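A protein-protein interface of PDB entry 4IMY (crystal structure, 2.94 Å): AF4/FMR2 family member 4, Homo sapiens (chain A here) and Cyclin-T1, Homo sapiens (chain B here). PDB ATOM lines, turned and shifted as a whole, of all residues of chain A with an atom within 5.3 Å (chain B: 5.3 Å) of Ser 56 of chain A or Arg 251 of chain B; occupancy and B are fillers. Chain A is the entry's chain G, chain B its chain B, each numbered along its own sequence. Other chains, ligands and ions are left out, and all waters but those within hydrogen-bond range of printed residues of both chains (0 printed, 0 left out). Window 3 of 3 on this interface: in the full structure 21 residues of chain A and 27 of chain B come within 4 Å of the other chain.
Ser 56 of chain A touches one residue of chain B. Arg 251 of chain B touches just these residues of chain A: Ser 56 (3.5 Å) and Met 57 (3.1 Å). Of the printed residues of chain A, Leu 245 of chain B touches Met 57 and Leu 58. Printed residues of chain B within 4 Å of Leu 58 of chain A: Leu 245 (3.4 Å). Printed residues of chain B within 4 Å of Met 57 of chain A: Leu 245 (3.4 Å), Glu 246 (3.0 Å) and Arg 251 (3.1 Å). Of the printed residues of chain A, Glu 246 of chain B touches Met 57. Thr 248 of chain B touches none of the printed residues of chain A.
Arg 251 of chain B touches Ser 56 of chain A. CB of Leu 245 of chain B touches CE of Met 57 of chain A (3.4 Å). Glu 246 of chain B touches Met 57 of chain A. CD2 of Leu 58 of chain A touches CD1 of Leu 245 of chain B, at 3.4 Å.
Hydrophobic or aromatic side chains of chain A within 4 Å of the printed part of chain B: Met 57 and Leu 58. Hydrophobic or aromatic side chains of chain B that line the printed part of chain A: Leu 245.
O of Leu 245 of chain B lies within hydrogen-bond range of OG1 of Thr 248 of chain B (2.8 Å). O of Ser 52 of chain A is in hydrogen-bond range of OG of Ser 56 of chain A (3.4 Å).
The backbone carbonyl oxygen (O) of Met 57 of chain A lies within hydrogen-bond range of the guanidinium group (NE) of Arg 251 of chain B, 3.1 Å away.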
ATOM      1  N   SER A  52      25.379 -15.672  -3.032  1.00  0.00           N
ATOM      2  CA  SER A  52      24.065 -16.077  -3.517  1.00  0.00           C
ATOM      3  C   SER A  52      23.484 -17.173  -2.631  1.00  0.00           C
ATOM      4  O   SER A  52      22.329 -17.097  -2.203  1.00  0.00           O
ATOM      5  CB  SER A  52      24.164 -16.581  -4.958  1.00  0.00           C
ATOM      6  OG  SER A  52      24.733 -15.600  -5.808  1.00  0.00           O
ATOM      7  N   ARG A  53      24.295 -18.189  -2.358  1.00  0.00           N
ATOM      8  CA  ARG A  53      23.877 -19.321  -1.540  1.00  0.00           C
ATOM      9  C   ARG A  53      23.548 -18.883  -0.116  1.00  0.00           C
ATOM     10  O   ARG A  53      22.559 -19.326   0.467  1.00  0.00           O
ATOM     11  CB  ARG A  53      24.978 -20.383  -1.512  1.00  0.00           C
ATOM     12  N   ILE A  54      24.383 -18.011   0.439  1.00  0.00           N
ATOM     13  CA  ILE A  54      24.193 -17.524   1.800  1.00  0.00           C
ATOM     14  C   ILE A  54      22.871 -16.776   1.934  1.00  0.00           C
ATOM     15  O   ILE A  54      22.160 -16.931   2.926  1.00  0.00           O
ATOM     16  CB  ILE A  54      25.340 -16.587   2.222  1.00  0.00           C
ATOM     17  CG1 ILE A  54      26.665 -17.349   2.256  1.00  0.00           C
ATOM     18  CG2 ILE A  54      25.069 -15.997   3.593  1.00  0.00           C
ATOM     19  CD1 ILE A  54      27.889 -16.459   2.234  1.00  0.00           C
ATOM     20  N   GLN A  55      22.547 -15.966   0.930  1.00  0.00           N
ATOM     21  CA  GLN A  55      21.316 -15.180   0.947  1.00  0.00           C
ATOM     22  C   GLN A  55      20.086 -16.082   1.050  1.00  0.00           C
ATOM     23  O   GLN A  55      19.013 -15.635   1.452  1.00  0.00           O
ATOM     24  CB  GLN A  55      21.224 -14.305  -0.305  1.00  0.00           C
ATOM     25  N   SER A  56      20.249 -17.351   0.689  1.00  0.00           N
ATOM     26  CA  SER A  56      19.155 -18.313   0.753  1.00  0.00           C
ATOM     27  C   SER A  56      19.235 -19.160   2.022  1.00  0.00           C
ATOM     28  O   SER A  56      18.213 -19.503   2.615  1.00  0.00           O
ATOM     29  CB  SER A  56      19.183 -19.218  -0.478  1.00  0.00           C
ATOM     30  OG  SER A  56      19.260 -18.450  -1.667  1.00  0.00           O
ATOM     31  N   MET A  57      20.454 -19.494   2.433  1.00  0.00           N
ATOM     32  CA  MET A  57      20.668 -20.327   3.612  1.00  0.00           C
ATOM     33  C   MET A  57      20.323 -19.591   4.907  1.00  0.00           C
ATOM     34  O   MET A  57      20.023 -20.223   5.921  1.00  0.00           O
ATOM     35  CB  MET A  57      22.124 -20.796   3.667  1.00  0.00           C
ATOM     36  CG  MET A  57      22.495 -21.838   2.617  1.00  0.00           C
ATOM     37  SD  MET A  57      21.478 -23.326   2.692  1.00  0.00           S
ATOM     38  CE  MET A  57      21.469 -23.603   4.460  1.00  0.00           C
ATOM     39  N   LEU A  58      20.381 -18.261   4.869  1.00  0.00           N
ATOM     40  CA  LEU A  58      20.116 -17.439   6.049  1.00  0.00           C
ATOM     41  C   LEU A  58      18.957 -16.463   5.842  1.00  0.00           C
ATOM     42  O   LEU A  58      18.442 -15.896   6.806  1.00  0.00           O
ATOM     43  CB  LEU A  58      21.367 -16.643   6.422  1.00  0.00           C
ATOM     44  CG  LEU A  58      22.668 -17.442   6.498  1.00  0.00           C
ATOM     45  CD1 LEU A  58      23.840 -16.528   6.820  1.00  0.00           C
ATOM     46  CD2 LEU A  58      22.560 -18.555   7.526  1.00  0.00           C
ATOM     47  N   GLY A  59      18.551 -16.267   4.590  1.00  0.00           N
ATOM     48  CA  GLY A  59      17.537 -15.282   4.265  1.00  0.00           C
ATOM     49  C   GLY A  59      18.183 -13.983   3.827  1.00  0.00           C
ATOM     50  O   GLY A  59      19.406 -13.852   3.875  1.00  0.00           O
ATOM     51  N   LEU B 245      24.103 -26.044   7.653  1.00  0.00           N
ATOM     52  CA  LEU B 245      22.824 -25.359   7.788  1.00  0.00           C
ATOM     53  C   LEU B 245      21.762 -25.989   6.890  1.00  0.00           C
ATOM     54  O   LEU B 245      20.624 -26.196   7.311  1.00  0.00           O
ATOM     55  CB  LEU B 245      22.978 -23.877   7.452  1.00  0.00           C
ATOM     56  CG  LEU B 245      23.786 -23.048   8.450  1.00  0.00           C
ATOM     57  CD1 LEU B 245      24.021 -21.649   7.906  1.00  0.00           C
ATOM     58  CD2 LEU B 245      23.082 -22.981   9.795  1.00  0.00           C
ATOM     59  N   GLU B 246      22.139 -26.295   5.652  1.00  0.00           N
ATOM     60  CA  GLU B 246      21.209 -26.886   4.692  1.00  0.00           C
ATOM     61  C   GLU B 246      20.576 -28.162   5.230  1.00  0.00           C
ATOM     62  O   GLU B 246      19.415 -28.453   4.940  1.00  0.00           O
ATOM     63  CB  GLU B 246      21.921 -27.176   3.368  1.00  0.00           C
ATOM     64  N   THR B 248      19.975 -28.909   8.395  1.00  0.00           N
ATOM     65  CA  THR B 248      19.163 -28.712   9.593  1.00  0.00           C
ATOM     66  C   THR B 248      17.690 -28.599   9.210  1.00  0.00           C
ATOM     67  O   THR B 248      17.349 -27.909   8.249  1.00  0.00           O
ATOM     68  CB  THR B 248      19.569 -27.450  10.379  1.00  0.00           C
ATOM     69  OG1 THR B 248      19.101 -26.282   9.696  1.00  0.00           O
ATOM     70  CG2 THR B 248      21.076 -27.378  10.547  1.00  0.00           C
ATOM     71  N   PRO B 249      16.811 -29.269   9.972  1.00  0.00           N
ATOM     72  CA  PRO B 249      15.383 -29.373   9.643  1.00  0.00           C
ATOM     73  C   PRO B 249      14.698 -28.020   9.454  1.00  0.00           C
ATOM     74  O   PRO B 249      14.513 -27.581   8.317  1.00  0.00           O
ATOM     75  CB  PRO B 249      14.793 -30.117  10.848  1.00  0.00           C
ATOM     76  CG  PRO B 249      15.802 -29.964  11.942  1.00  0.00           C
ATOM     77  CD  PRO B 249      17.126 -29.907  11.261  1.00  0.00           C
ATOM     78  N   ASN B 250      14.319 -27.376  10.552  1.00  0.00           N
ATOM     79  CA  ASN B 250      13.679 -26.073  10.482  1.00  0.00           C
ATOM     80  C   ASN B 250      14.671 -24.977  10.833  1.00  0.00           C
ATOM     81  O   ASN B 250      15.102 -24.865  11.980  1.00  0.00           O
ATOM     82  CB  ASN B 250      12.481 -26.015  11.431  1.00  0.00           C
ATOM     83  N   ARG B 251      15.030 -24.166   9.843  1.00  0.00           N
ATOM     84  CA  ARG B 251      15.967 -23.071  10.069  1.00  0.00           C
ATOM     85  C   ARG B 251      15.254 -21.862  10.668  1.00  0.00           C
ATOM     86  O   ARG B 251      15.691 -20.722  10.512  1.00  0.00           O
ATOM     87  CB  ARG B 251      16.689 -22.703   8.775  1.00  0.00           C
ATOM     88  CG  ARG B 251      17.447 -23.874   8.177  1.00  0.00           C
ATOM     89  CD  ARG B 251      18.606 -23.424   7.309  1.00  0.00           C
ATOM     90  NE  ARG B 251      18.170 -22.741   6.095  1.00  0.00           N
ATOM     91  CZ  ARG B 251      17.720 -23.357   5.006  1.00  0.00           C
ATOM     92  NH1 ARG B 251      17.627 -24.681   4.971  1.00  0.00           N
ATOM     93  NH2 ARG B 251      17.352 -22.646   3.951  1.00  0.00           N
ATOM     94  N   LEU B 252      14.137 -22.129  11.337  1.00  0.00           N
ATOM     95  CA  LEU B 252      13.555 -21.189  12.279  1.00  0.00           C
ATOM     96  C   LEU B 252      14.385 -21.222  13.556  1.00  0.00           C
ATOM     97  O   LEU B 252      14.176 -20.424  14.466  1.00  0.00           O
ATOM     98  CB  LEU B 252      12.111 -21.578  12.598  1.00  0.00           C
ATOM     99  N   LYS B 253      15.305 -22.181  13.629  1.00  0.00           N
ATOM    100  CA  LYS B 253      16.201 -22.300  14.769  1.00  0.00           C
ATOM    101  C   LYS B 253      17.310 -21.258  14.675  1.00  0.00           C
ATOM    102  O   LYS B 253      17.802 -20.770  15.694  1.00  0.00           O
ATOM    103  CB  LYS B 253      16.805 -23.703  14.829  1.00  0.00           C
ATOM    104  N   ARG B 254      17.703 -20.922  13.450  1.00  0.00           N
ATOM    105  CA  ARG B 254      18.732 -19.915  13.230  1.00  0.00           C
ATOM    106  C   ARG B 254      18.231 -18.556  13.686  1.00  0.00           C
ATOM    107  O   ARG B 254      18.651 -18.039  14.721  1.00  0.00           O
ATOM    108  CB  ARG B 254      19.124 -19.853  11.751  1.00  0.00           C
ATOM    109  N   ILE B 255      17.314 -17.990  12.910  1.00  0.00           N
ATOM    110  CA  ILE B 255      16.822 -16.640  13.154  1.00  0.00           C
ATOM    111  C   ILE B 255      15.965 -16.551  14.426  1.00  0.00           C
ATOM    112  O   ILE B 255      15.709 -15.457  14.931  1.00  0.00           O
ATOM    113  CB  ILE B 255      16.040 -16.113  11.921  1.00  0.00           C
ATOM    114  CG1 ILE B 255      17.015 -15.688  10.812  1.00  0.00           C
ATOM    115  CG2 ILE B 255      15.127 -14.957  12.306  1.00  0.00           C
ATOM    116  CD1 ILE B 255      17.892 -14.471  11.156  1.00  0.00           C
